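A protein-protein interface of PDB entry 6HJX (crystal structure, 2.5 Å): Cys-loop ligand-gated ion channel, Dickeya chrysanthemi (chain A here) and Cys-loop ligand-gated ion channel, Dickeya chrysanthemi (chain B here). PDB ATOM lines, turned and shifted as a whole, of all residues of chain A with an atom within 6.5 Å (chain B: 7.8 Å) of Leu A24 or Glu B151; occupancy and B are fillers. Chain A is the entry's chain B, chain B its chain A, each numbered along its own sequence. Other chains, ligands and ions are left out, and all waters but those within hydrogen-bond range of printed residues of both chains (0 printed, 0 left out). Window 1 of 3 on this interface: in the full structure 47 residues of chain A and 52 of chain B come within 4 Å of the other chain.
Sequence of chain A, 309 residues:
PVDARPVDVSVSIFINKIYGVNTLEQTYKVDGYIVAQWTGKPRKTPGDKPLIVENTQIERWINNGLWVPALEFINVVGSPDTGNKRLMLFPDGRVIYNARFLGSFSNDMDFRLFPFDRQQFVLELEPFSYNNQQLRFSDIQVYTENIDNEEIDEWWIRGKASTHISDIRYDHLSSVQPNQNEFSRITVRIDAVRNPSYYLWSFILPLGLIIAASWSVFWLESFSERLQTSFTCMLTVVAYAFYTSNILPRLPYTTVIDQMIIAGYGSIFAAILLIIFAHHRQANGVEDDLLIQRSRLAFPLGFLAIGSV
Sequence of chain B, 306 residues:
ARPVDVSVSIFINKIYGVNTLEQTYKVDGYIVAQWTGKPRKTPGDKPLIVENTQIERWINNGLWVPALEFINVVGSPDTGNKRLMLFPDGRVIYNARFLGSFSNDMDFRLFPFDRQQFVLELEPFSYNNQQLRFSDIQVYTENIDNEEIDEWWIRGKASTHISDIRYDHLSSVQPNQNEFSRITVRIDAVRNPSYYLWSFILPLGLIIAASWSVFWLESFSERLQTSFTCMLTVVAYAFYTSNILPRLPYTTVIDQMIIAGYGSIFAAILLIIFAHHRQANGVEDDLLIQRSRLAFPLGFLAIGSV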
ATOM      1  N   ASN A  22       0.942 -23.879   9.292  1.00  0.00           N
ATOM      2  CA  ASN A  22       0.022 -24.314  10.342  1.00  0.00           C
ATOM      3  C   ASN A  22      -1.144 -25.002   9.635  1.00  0.00           C
ATOM      4  O   ASN A  22      -2.039 -24.336   9.104  1.00  0.00           O
ATOM      5  CB  ASN A  22      -0.434 -23.136  11.195  1.00  0.00           C
ATOM      6  CG  ASN A  22      -1.326 -23.556  12.348  1.00  0.00           C
ATOM      7  OD1 ASN A  22      -2.186 -24.420  12.199  1.00  0.00           O
ATOM      8  ND2 ASN A  22      -1.126 -22.939  13.504  1.00  0.00           N
ATOM      9  N   THR A  23      -1.128 -26.336   9.628  1.00  0.00           N
ATOM     10  CA  THR A  23      -2.068 -27.086   8.801  1.00  0.00           C
ATOM     11  C   THR A  23      -3.513 -26.808   9.191  1.00  0.00           C
ATOM     12  O   THR A  23      -4.376 -26.647   8.322  1.00  0.00           O
ATOM     13  CB  THR A  23      -1.769 -28.581   8.901  1.00  0.00           C
ATOM     14  OG1 THR A  23      -1.521 -28.931  10.268  1.00  0.00           O
ATOM     15  CG2 THR A  23      -0.556 -28.941   8.058  1.00  0.00           C
ATOM     16  N   LEU A  24      -3.800 -26.745  10.493  1.00  0.00           N
ATOM     17  CA  LEU A  24      -5.184 -26.584  10.930  1.00  0.00           C
ATOM     18  C   LEU A  24      -5.718 -25.199  10.576  1.00  0.00           C
ATOM     19  O   LEU A  24      -6.866 -25.065  10.135  1.00  0.00           O
ATOM     20  CB  LEU A  24      -5.287 -26.838  12.434  1.00  0.00           C
ATOM     21  CG  LEU A  24      -6.679 -27.184  12.971  1.00  0.00           C
ATOM     22  CD1 LEU A  24      -7.199 -28.487  12.377  1.00  0.00           C
ATOM     23  CD2 LEU A  24      -6.655 -27.265  14.488  1.00  0.00           C
ATOM     24  N   GLU A  25      -4.900 -24.159  10.753  1.00  0.00           N
ATOM     25  CA  GLU A  25      -5.312 -22.800  10.427  1.00  0.00           C
ATOM     26  C   GLU A  25      -5.140 -22.467   8.950  1.00  0.00           C
ATOM     27  O   GLU A  25      -5.603 -21.408   8.515  1.00  0.00           O
ATOM     28  CB  GLU A  25      -4.525 -21.796  11.276  1.00  0.00           C
ATOM     29  CG  GLU A  25      -4.694 -21.996  12.770  1.00  0.00           C
ATOM     30  CD  GLU A  25      -4.002 -20.927  13.589  1.00  0.00           C
ATOM     31  OE1 GLU A  25      -3.195 -20.164  13.015  1.00  0.00           O
ATOM     32  OE2 GLU A  25      -4.271 -20.850  14.807  1.00  0.00           O
ATOM     33  N   GLN A  26      -4.505 -23.344   8.174  1.00  0.00           N
ATOM     34  CA  GLN A  26      -4.242 -23.095   6.758  1.00  0.00           C
ATOM     35  C   GLN A  26      -3.545 -21.749   6.563  1.00  0.00           C
ATOM     36  O   GLN A  26      -3.964 -20.908   5.766  1.00  0.00           O
ATOM     37  CB  GLN A  26      -5.533 -23.176   5.943  1.00  0.00           C
ATOM     38  CG  GLN A  26      -6.123 -24.584   5.861  1.00  0.00           C
ATOM     39  CD  GLN A  26      -7.408 -24.646   5.058  1.00  0.00           C
ATOM     40  OE1 GLN A  26      -7.427 -24.349   3.866  1.00  0.00           O
ATOM     41  NE2 GLN A  26      -8.490 -25.037   5.712  1.00  0.00           N
ATOM     42  N   THR A  27      -2.461 -21.552   7.312  1.00  0.00           N
ATOM     43  CA  THR A  27      -1.643 -20.353   7.207  1.00  0.00           C
ATOM     44  C   THR A  27      -0.185 -20.748   6.992  1.00  0.00           C
ATOM     45  O   THR A  27       0.185 -21.925   7.036  1.00  0.00           O
ATOM     46  CB  THR A  27      -1.775 -19.466   8.456  1.00  0.00           C
ATOM     47  OG1 THR A  27      -1.326 -20.180   9.616  1.00  0.00           O
ATOM     48  CG2 THR A  27      -3.215 -19.032   8.660  1.00  0.00           C
ATOM     49  N   PHE A 111      -4.380 -31.105   2.504  1.00  0.00           N
ATOM     50  CA  PHE A 111      -3.319 -31.997   2.954  1.00  0.00           C
ATOM     51  C   PHE A 111      -3.741 -33.461   2.935  1.00  0.00           C
ATOM     52  O   PHE A 111      -3.107 -34.292   3.595  1.00  0.00           O
ATOM     53  CB  PHE A 111      -2.863 -31.607   4.359  1.00  0.00           C
ATOM     54  CG  PHE A 111      -2.324 -30.208   4.459  1.00  0.00           C
ATOM     55  CD1 PHE A 111      -0.992 -29.943   4.184  1.00  0.00           C
ATOM     56  CD2 PHE A 111      -3.145 -29.162   4.842  1.00  0.00           C
ATOM     57  CE1 PHE A 111      -0.491 -28.656   4.281  1.00  0.00           C
ATOM     58  CE2 PHE A 111      -2.651 -27.872   4.943  1.00  0.00           C
ATOM     59  CZ  PHE A 111      -1.322 -27.619   4.659  1.00  0.00           C
ATOM     60  N   PRO A 249       0.967 -33.490  11.587  1.00  0.00           N
ATOM     61  CA  PRO A 249       0.182 -32.264  11.754  1.00  0.00           C
ATOM     62  C   PRO A 249      -1.293 -32.551  11.978  1.00  0.00           C
ATOM     63  O   PRO A 249      -1.862 -33.500  11.432  1.00  0.00           O
ATOM     64  CB  PRO A 249       0.405 -31.525  10.429  1.00  0.00           C
ATOM     65  CG  PRO A 249       0.630 -32.614   9.438  1.00  0.00           C
ATOM     66  CD  PRO A 249       1.363 -33.706  10.182  1.00  0.00           C
ATOM     67  N   ARG A 250      -1.914 -31.705  12.796  1.00  0.00           N
ATOM     68  CA  ARG A 250      -3.340 -31.834  13.057  1.00  0.00           C
ATOM     69  C   ARG A 250      -4.144 -31.455  11.821  1.00  0.00           C
ATOM     70  O   ARG A 250      -3.816 -30.501  11.110  1.00  0.00           O
ATOM     71  CB  ARG A 250      -3.748 -30.956  14.238  1.00  0.00           C
ATOM     72  CG  ARG A 250      -3.065 -31.312  15.554  1.00  0.00           C
ATOM     73  CD  ARG A 250      -3.474 -32.693  16.080  1.00  0.00           C
ATOM     74  NE  ARG A 250      -2.576 -33.757  15.624  1.00  0.00           N
ATOM     75  CZ  ARG A 250      -2.917 -34.762  14.814  1.00  0.00           C
ATOM     76  NH1 ARG A 250      -4.156 -34.879  14.343  1.00  0.00           N
ATOM     77  NH2 ARG A 250      -2.004 -35.663  14.474  1.00  0.00           N
ATOM     78  N   LEU A 251      -5.207 -32.214  11.567  1.00  0.00           N
ATOM     79  CA  LEU A 251      -6.022 -32.030  10.378  1.00  0.00           C
ATOM     80  C   LEU A 251      -7.459 -32.406  10.697  1.00  0.00           C
ATOM     81  O   LEU A 251      -7.697 -33.227  11.594  1.00  0.00           O
ATOM     82  CB  LEU A 251      -5.507 -32.884   9.210  1.00  0.00           C
ATOM     83  CG  LEU A 251      -4.135 -32.512   8.654  1.00  0.00           C
ATOM     84  CD1 LEU A 251      -3.654 -33.584   7.698  1.00  0.00           C
ATOM     85  CD2 LEU A 251      -4.190 -31.160   7.959  1.00  0.00           C
ATOM     86  N   PRO A 252      -8.429 -31.824  10.000  1.00  0.00           N
ATOM     87  CA  PRO A 252      -9.828 -32.267  10.135  1.00  0.00           C
ATOM     88  C   PRO A 252     -10.201 -33.444   9.246  1.00  0.00           C
ATOM     89  O   PRO A 252     -11.392 -33.744   9.125  1.00  0.00           O
ATOM     90  CB  PRO A 252     -10.608 -31.010   9.725  1.00  0.00           C
ATOM     91  CG  PRO A 252      -9.733 -30.355   8.711  1.00  0.00           C
ATOM     92  CD  PRO A 252      -8.312 -30.635   9.134  1.00  0.00           C
ATOM     93  N   LYS B  14     -12.554 -15.103   7.850  1.00  0.00           N
ATOM     94  CA  LYS B  14     -12.061 -16.354   8.403  1.00  0.00           C
ATOM     95  C   LYS B  14     -12.489 -16.456   9.859  1.00  0.00           C
ATOM     96  O   LYS B  14     -12.485 -15.457  10.582  1.00  0.00           O
ATOM     97  CB  LYS B  14     -10.533 -16.412   8.277  1.00  0.00           C
ATOM     98  CG  LYS B  14      -9.909 -17.775   8.454  1.00  0.00           C
ATOM     99  CD  LYS B  14      -8.384 -17.664   8.381  1.00  0.00           C
ATOM    100  CE  LYS B  14      -7.703 -19.020   8.490  1.00  0.00           C
ATOM    101  NZ  LYS B  14      -8.042 -19.901   7.338  1.00  0.00           N
ATOM    102  N   ILE B  15     -12.876 -17.662  10.271  1.00  0.00           N
ATOM    103  CA  ILE B  15     -13.107 -17.990  11.674  1.00  0.00           C
ATOM    104  C   ILE B  15     -12.331 -19.263  11.965  1.00  0.00           C
ATOM    105  O   ILE B  15     -12.623 -20.317  11.389  1.00  0.00           O
ATOM    106  CB  ILE B  15     -14.596 -18.184  12.003  1.00  0.00           C
ATOM    107  CG1 ILE B  15     -15.391 -16.933  11.642  1.00  0.00           C
ATOM    108  CG2 ILE B  15     -14.767 -18.508  13.488  1.00  0.00           C
ATOM    109  CD1 ILE B  15     -16.888 -17.077  11.849  1.00  0.00           C
ATOM    110  N   TYR B  16     -11.360 -19.174  12.864  1.00  0.00           N
ATOM    111  CA  TYR B  16     -10.420 -20.264  13.080  1.00  0.00           C
ATOM    112  C   TYR B  16      -9.849 -20.137  14.485  1.00  0.00           C
ATOM    113  O   TYR B  16     -10.216 -19.241  15.251  1.00  0.00           O
ATOM    114  CB  TYR B  16      -9.310 -20.231  12.027  1.00  0.00           C
ATOM    115  CG  TYR B  16      -8.375 -19.062  12.218  1.00  0.00           C
ATOM    116  CD1 TYR B  16      -8.748 -17.779  11.843  1.00  0.00           C
ATOM    117  CD2 TYR B  16      -7.127 -19.240  12.791  1.00  0.00           C
ATOM    118  CE1 TYR B  16      -7.898 -16.708  12.025  1.00  0.00           C
ATOM    119  CE2 TYR B  16      -6.269 -18.179  12.976  1.00  0.00           C
ATOM    120  CZ  TYR B  16      -6.659 -16.914  12.593  1.00  0.00           C
ATOM    121  OH  TYR B  16      -5.810 -15.849  12.783  1.00  0.00           O
ATOM    122  N   GLY B  17      -8.936 -21.045  14.814  1.00  0.00           N
ATOM    123  CA  GLY B  17      -8.192 -20.952  16.058  1.00  0.00           C
ATOM    124  C   GLY B  17      -9.049 -21.093  17.294  1.00  0.00           C
ATOM    125  O   GLY B  17      -8.817 -20.398  18.290  1.00  0.00           O
ATOM    126  N   VAL B  18     -10.043 -21.980  17.253  1.00  0.00           N
ATOM    127  CA  VAL B  18     -10.872 -22.219  18.425  1.00  0.00           C
ATOM    128  C   VAL B  18      -9.994 -22.674  19.582  1.00  0.00           C
ATOM    129  O   VAL B  18      -9.136 -23.553  19.432  1.00  0.00           O
ATOM    130  CB  VAL B  18     -11.961 -23.254  18.103  1.00  0.00           C
ATOM    131  CG1 VAL B  18     -12.663 -23.715  19.375  1.00  0.00           C
ATOM    132  CG2 VAL B  18     -12.970 -22.672  17.125  1.00  0.00           C
ATOM    133  N   THR B  20     -10.778 -24.406  23.003  1.00  0.00           N
ATOM    134  CA  THR B  20     -11.911 -25.048  23.659  1.00  0.00           C
ATOM    135  C   THR B  20     -11.967 -24.711  25.143  1.00  0.00           C
ATOM    136  O   THR B  20     -13.046 -24.444  25.684  1.00  0.00           O
ATOM    137  CB  THR B  20     -11.840 -26.563  23.463  1.00  0.00           C
ATOM    138  OG1 THR B  20     -10.545 -27.041  23.851  1.00  0.00           O
ATOM    139  CG2 THR B  20     -12.101 -26.920  22.009  1.00  0.00           C
ATOM    140  N   PHE B 111     -19.029 -33.552  21.388  1.00  0.00           N
ATOM    141  CA  PHE B 111     -17.894 -33.744  20.499  1.00  0.00           C
ATOM    142  C   PHE B 111     -17.821 -35.207  20.065  1.00  0.00           C
ATOM    143  O   PHE B 111     -18.067 -36.106  20.879  1.00  0.00           O
ATOM    144  CB  PHE B 111     -16.604 -33.331  21.217  1.00  0.00           C
ATOM    145  CG  PHE B 111     -15.364 -33.466  20.380  1.00  0.00           C
ATOM    146  CD1 PHE B 111     -14.657 -34.657  20.353  1.00  0.00           C
ATOM    147  CD2 PHE B 111     -14.895 -32.398  19.635  1.00  0.00           C
ATOM    148  CE1 PHE B 111     -13.510 -34.785  19.590  1.00  0.00           C
ATOM    149  CE2 PHE B 111     -13.750 -32.517  18.869  1.00  0.00           C
ATOM    150  CZ  PHE B 111     -13.056 -33.714  18.848  1.00  0.00           C
ATOM    151  N   PRO B 112     -17.484 -35.494  18.794  1.00  0.00           N
ATOM    152  CA  PRO B 112     -17.137 -34.583  17.697  1.00  0.00           C
ATOM    153  C   PRO B 112     -18.323 -34.147  16.837  1.00  0.00           C
ATOM    154  O   PRO B 112     -18.131 -33.805  15.670  1.00  0.00           O
ATOM    155  CB  PRO B 112     -16.163 -35.421  16.869  1.00  0.00           C
ATOM    156  CG  PRO B 112     -16.690 -36.814  17.017  1.00  0.00           C
ATOM    157  CD  PRO B 112     -17.285 -36.903  18.408  1.00  0.00           C
ATOM    158  N   GLU B 147     -16.601 -27.724   1.269  1.00  0.00           N
ATOM    159  CA  GLU B 147     -16.402 -27.721   2.714  1.00  0.00           C
ATOM    160  C   GLU B 147     -15.772 -29.009   3.243  1.00  0.00           C
ATOM    161  O   GLU B 147     -15.750 -29.206   4.463  1.00  0.00           O
ATOM    162  CB  GLU B 147     -17.740 -27.479   3.424  1.00  0.00           C
ATOM    163  CG  GLU B 147     -18.792 -28.558   3.189  1.00  0.00           C
ATOM    164  CD  GLU B 147     -20.107 -28.258   3.893  1.00  0.00           C
ATOM    165  OE1 GLU B 147     -20.260 -27.137   4.427  1.00  0.00           O
ATOM    166  OE2 GLU B 147     -20.988 -29.144   3.912  1.00  0.00           O
ATOM    167  N   GLU B 148     -15.253 -29.878   2.372  1.00  0.00           N
ATOM    168  CA  GLU B 148     -14.715 -31.155   2.831  1.00  0.00           C
ATOM    169  C   GLU B 148     -13.367 -30.996   3.524  1.00  0.00           C
ATOM    170  O   GLU B 148     -13.039 -31.784   4.417  1.00  0.00           O
ATOM    171  CB  GLU B 148     -14.585 -32.123   1.654  1.00  0.00           C
ATOM    172  N   ILE B 149     -12.576 -29.996   3.137  1.00  0.00           N
ATOM    173  CA  ILE B 149     -11.238 -29.829   3.694  1.00  0.00           C
ATOM    174  C   ILE B 149     -11.259 -28.856   4.869  1.00  0.00           C
ATOM    175  O   ILE B 149     -10.203 -28.421   5.345  1.00  0.00           O
ATOM    176  CB  ILE B 149     -10.238 -29.346   2.621  1.00  0.00           C
ATOM    177  CG1 ILE B 149     -10.628 -27.962   2.086  1.00  0.00           C
ATOM    178  CG2 ILE B 149     -10.162 -30.344   1.472  1.00  0.00           C
ATOM    179  CD1 ILE B 149      -9.434 -27.071   1.767  1.00  0.00           C
ATOM    180  N   ASP B 150     -12.451 -28.504   5.344  1.00  0.00           N
ATOM    181  CA  ASP B 150     -12.608 -27.464   6.351  1.00  0.00           C
ATOM    182  C   ASP B 150     -12.994 -28.066   7.696  1.00  0.00           C
ATOM    183  O   ASP B 150     -13.744 -29.045   7.763  1.00  0.00           O
ATOM    184  CB  ASP B 150     -13.656 -26.437   5.911  1.00  0.00           C
ATOM    185  CG  ASP B 150     -13.186 -25.592   4.740  1.00  0.00           C
ATOM    186  OD1 ASP B 150     -11.978 -25.272   4.681  1.00  0.00           O
ATOM    187  OD2 ASP B 150     -14.023 -25.251   3.876  1.00  0.00           O
ATOM    188  N   GLU B 151     -12.474 -27.462   8.767  1.00  0.00           N
ATOM    189  CA  GLU B 151     -12.732 -27.959  10.114  1.00  0.00           C
ATOM    190  C   GLU B 151     -14.187 -27.763  10.521  1.00  0.00           C
ATOM    191  O   GLU B 151     -14.737 -28.594  11.254  1.00  0.00           O
ATOM    192  CB  GLU B 151     -11.800 -27.256  11.103  1.00  0.00           C
ATOM    193  CG  GLU B 151     -11.875 -27.769  12.532  1.00  0.00           C
ATOM    194  CD  GLU B 151     -10.822 -27.138  13.430  1.00  0.00           C
ATOM    195  OE1 GLU B 151     -10.020 -26.316  12.930  1.00  0.00           O
ATOM    196  OE2 GLU B 151     -10.798 -27.459  14.637  1.00  0.00           O
ATOM    197  N   TRP B 152     -14.826 -26.690  10.059  1.00  0.00           N
ATOM    198  CA  TRP B 152     -16.191 -26.361  10.445  1.00  0.00           C
ATOM    199  C   TRP B 152     -17.052 -26.203   9.203  1.00  0.00           C
ATOM    200  O   TRP B 152     -16.591 -25.728   8.165  1.00  0.00           O
ATOM    201  CB  TRP B 152     -16.237 -25.075  11.278  1.00  0.00           C
ATOM    202  CG  TRP B 152     -15.645 -25.239  12.635  1.00  0.00           C
ATOM    203  CD1 TRP B 152     -14.375 -24.933  13.016  1.00  0.00           C
ATOM    204  CD2 TRP B 152     -16.301 -25.761  13.796  1.00  0.00           C
ATOM    205  NE1 TRP B 152     -14.197 -25.228  14.346  1.00  0.00           N
ATOM    206  CE2 TRP B 152     -15.366 -25.738  14.848  1.00  0.00           C
ATOM    207  CE3 TRP B 152     -17.590 -26.243  14.050  1.00  0.00           C
ATOM    208  CZ2 TRP B 152     -15.675 -26.181  16.132  1.00  0.00           C
ATOM    209  CZ3 TRP B 152     -17.896 -26.680  15.325  1.00  0.00           C
ATOM    210  CH2 TRP B 152     -16.942 -26.647  16.350  1.00  0.00           C
ATOM    211  N   TRP B 153     -18.314 -26.610   9.321  1.00  0.00           N
ATOM    212  CA  TRP B 153     -19.278 -26.518   8.232  1.00  0.00           C
ATOM    213  C   TRP B 153     -20.320 -25.464   8.584  1.00  0.00           C
ATOM    214  O   TRP B 153     -21.075 -25.633   9.547  1.00  0.00           O
ATOM    215  CB  TRP B 153     -19.950 -27.867   7.984  1.00  0.00           C
ATOM    216  CG  TRP B 153     -19.038 -28.921   7.452  1.00  0.00           C
ATOM    217  CD1 TRP B 153     -17.791 -28.746   6.928  1.00  0.00           C
ATOM    218  CD2 TRP B 153     -19.306 -30.326   7.393  1.00  0.00           C
ATOM    219  NE1 TRP B 153     -17.265 -29.957   6.546  1.00  0.00           N
ATOM    220  CE2 TRP B 153     -18.176 -30.942   6.820  1.00  0.00           C
ATOM    221  CE3 TRP B 153     -20.391 -31.122   7.771  1.00  0.00           C
ATOM    222  CZ2 TRP B 153     -18.102 -32.317   6.616  1.00  0.00           C
ATOM    223  CZ3 TRP B 153     -20.315 -32.484   7.568  1.00  0.00           C
ATOM    224  CH2 TRP B 153     -19.179 -33.069   6.996  1.00  0.00           C
ATOM    225  N   ILE B 154     -20.363 -24.389   7.801  1.00  0.00           N
ATOM    226  CA  ILE B 154     -21.304 -23.302   8.042  1.00  0.00           C
ATOM    227  C   ILE B 154     -22.694 -23.736   7.596  1.00  0.00           C
ATOM    228  O   ILE B 154     -22.858 -24.374   6.550  1.00  0.00           O
ATOM    229  CB  ILE B 154     -20.851 -22.023   7.313  1.00  0.00           C
ATOM    230  CG1 ILE B 154     -19.764 -21.300   8.114  1.00  0.00           C
ATOM    231  CG2 ILE B 154     -22.024 -21.072   7.095  1.00  0.00           C
ATOM    232  CD1 ILE B 154     -18.505 -22.095   8.311  1.00  0.00           C
ATOM    233  N   ALA B 189     -22.410 -23.139  12.875  1.00  0.00           N
ATOM    234  CA  ALA B 189     -21.458 -24.068  12.281  1.00  0.00           C
ATOM    235  C   ALA B 189     -21.508 -25.401  13.010  1.00  0.00           C
ATOM    236  O   ALA B 189     -21.701 -25.444  14.227  1.00  0.00           O
ATOM    237  CB  ALA B 189     -20.034 -23.502  12.325  1.00  0.00           C
ATOM    238  N   VAL B 190     -21.336 -26.486  12.254  1.00  0.00           N
ATOM    239  CA  VAL B 190     -21.197 -27.824  12.817  1.00  0.00           C
ATOM    240  C   VAL B 190     -19.785 -28.316  12.529  1.00  0.00           C
ATOM    241  O   VAL B 190     -19.194 -27.995  11.491  1.00  0.00           O
ATOM    242  CB  VAL B 190     -22.242 -28.816  12.259  1.00  0.00           C
ATOM    243  CG1 VAL B 190     -23.635 -28.210  12.308  1.00  0.00           C
ATOM    244  CG2 VAL B 190     -21.898 -29.234  10.838  1.00  0.00           C
ATOM    245  N   ARG B 191     -19.245 -29.102  13.454  1.00  0.00           N
ATOM    246  CA  ARG B 191     -17.897 -29.626  13.286  1.00  0.00           C
ATOM    247  C   ARG B 191     -17.882 -30.716  12.224  1.00  0.00           C
ATOM    248  O   ARG B 191     -18.839 -31.485  12.086  1.00  0.00           O
ATOM    249  CB  ARG B 191     -17.365 -30.180  14.609  1.00  0.00           C
ATOM    250  CG  ARG B 191     -15.893 -30.590  14.558  1.00  0.00           C
ATOM    251  CD  ARG B 191     -15.441 -31.255  15.849  1.00  0.00           C
ATOM    252  NE  ARG B 191     -15.740 -30.439  17.022  1.00  0.00           N
ATOM    253  CZ  ARG B 191     -14.963 -29.463  17.482  1.00  0.00           C
ATOM    254  NH1 ARG B 191     -13.824 -29.166  16.874  1.00  0.00           N
ATOM    255  NH2 ARG B 191     -15.329 -28.783  18.558  1.00  0.00           N
ATOM    256  N   ASN B 192     -16.789 -30.772  11.466  1.00  0.00           N
ATOM    257  CA  ASN B 192     -16.571 -31.830  10.488  1.00  0.00           C
ATOM    258  C   ASN B 192     -16.024 -33.058  11.210  1.00  0.00           C
ATOM    259  O   ASN B 192     -14.851 -33.068  11.603  1.00  0.00           O
ATOM    260  CB  ASN B 192     -15.604 -31.365   9.398  1.00  0.00           C
ATOM    261  CG  ASN B 192     -15.328 -32.442   8.368  1.00  0.00           C
ATOM    262  OD1 ASN B 192     -15.975 -33.488   8.361  1.00  0.00           O
ATOM    263  ND2 ASN B 192     -14.368 -32.185   7.485  1.00  0.00           N
ATOM    264  N   PRO B 193     -16.824 -34.107  11.401  1.00  0.00           N
ATOM    265  CA  PRO B 193     -16.417 -35.220  12.270  1.00  0.00           C
ATOM    266  C   PRO B 193     -15.718 -36.377  11.572  1.00  0.00           C
ATOM    267  O   PRO B 193     -15.542 -37.424  12.202  1.00  0.00           O
ATOM    268  CB  PRO B 193     -17.767 -35.685  12.827  1.00  0.00           C
ATOM    269  CG  PRO B 193     -18.688 -35.520  11.655  1.00  0.00           C
ATOM    270  CD  PRO B 193     -18.179 -34.328  10.859  1.00  0.00           C
ATOM    271  N   SER B 194     -15.321 -36.233  10.306  1.00  0.00           N
ATOM    272  CA  SER B 194     -14.809 -37.377   9.558  1.00  0.00           C
ATOM    273  C   SER B 194     -13.570 -37.960  10.227  1.00  0.00           C
ATOM    274  O   SER B 194     -13.528 -39.151  10.555  1.00  0.00           O
ATOM    275  CB  SER B 194     -14.506 -36.967   8.114  1.00  0.00           C
ATOM    276  OG  SER B 194     -13.511 -35.961   8.066  1.00  0.00           O
ATOM    277  N   TYR B 196     -12.437 -37.839  13.174  1.00  0.00           N
ATOM    278  CA  TYR B 196     -12.664 -38.451  14.478  1.00  0.00           C
ATOM    279  C   TYR B 196     -13.449 -39.751  14.367  1.00  0.00           C
ATOM    280  O   TYR B 196     -13.242 -40.668  15.168  1.00  0.00           O
ATOM    281  CB  TYR B 196     -13.386 -37.466  15.396  1.00  0.00           C
ATOM    282  CG  TYR B 196     -12.710 -36.120  15.466  1.00  0.00           C
ATOM    283  CD1 TYR B 196     -11.557 -35.941  16.218  1.00  0.00           C
ATOM    284  CD2 TYR B 196     -13.218 -35.028  14.775  1.00  0.00           C
ATOM    285  CE1 TYR B 196     -10.931 -34.716  16.281  1.00  0.00           C
ATOM    286  CE2 TYR B 196     -12.600 -33.797  14.833  1.00  0.00           C
ATOM    287  CZ  TYR B 196     -11.457 -33.646  15.589  1.00  0.00           C
ATOM    288  OH  TYR B 196     -10.836 -32.421  15.652  1.00  0.00           O
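The side-chain hydroxyl (OG) of Ser B194 is in hydrogen-bond range of the backbone carbonyl oxygen (O) of Pro A252 (3.2 Å).
O of Glu A25 lies within hydrogen-bond range of NZ of Lys B14.
CG of Leu A24 touches OE1 of Glu B151, at 3.5 Å.
CD of Glu A25 touches CE2 of Tyr B16, at 3.6 Å.
Ile B149 touches Gln A26.
Asp B150 touches Gln A26.
Pro A252 touches Ile B149 (CG to O, 3.9 Å).
Glu B151 touches Pro A252.
Asn B192 touches Pro A252 (ND2 to O, 3.7 Å).
Of chain B, only Glu B151 comes within 4 Å of Leu A24.
Of the printed residues of chain B, Pro A252 touches Ile B149 (3.9 Å), Glu B151 (3.7 Å), Asn B192 (3.7 Å) and Ser B194 (3.2 Å).
Val B18 touches none of the printed residues of chain A.
Glu B147 touches none of the printed residues of chain A.
Of the printed residues of chain A, Asp B150 touches Gln A26 (3.6 Å).
Of chain A, only Leu A24 and Pro A252 come within 4 Å of Glu B151.
The nearest residue of chain A that does not touch Glu B151 is Gln A26 (5.6 Å).
The nearest printed residue of chain A that does not touch Asn B192 is Leu A251 (7.2 Å).
Of the 23 printed residues of chain B, 7 touch a printed residue of chain A.
Along chain B the printed residues that touch a printed residue of chain A span positions 14 to 194.
Of the 11 printed residues of chain A, 4 touch a printed residue of chain B.
Hydrophobic or aromatic side chains of chain A within 4 Å of the printed part of chain B: Leu A24 and Pro A252.
Among the printed residues, no Asp or Glu carboxylate lies within 4 Å of a Lys or Arg side-chain nitrogen of the other chain.
The backbone carbonyl oxygen (O) of Glu B148 sits at hydrogen-bond distance from the side-chain amide nitrogen (ND2) of Asn B192, 3.4 Å away.
The side-chain amide nitrogen (ND2) of Asn B192 lies within hydrogen-bond range of the backbone carbonyl oxygen (O) of Asp B150 (3.2 Å).
The backbone NH of Leu A24 lies close to the side-chain amide oxygen of Asn A22 (3.3 Å).
The backbone carbonyl oxygen (O) of Glu B151 sits at hydrogen-bond distance from the backbone NH (N) of Asn B192 (3.0 Å).
N of Ser B194 lies close to OD1 of Asn B192, 3.4 Å away.
The backbone NH (N) of Glu A25 sits at hydrogen-bond distance from the side-chain amide oxygen (OD1) of Asn A22 (3.1 Å).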
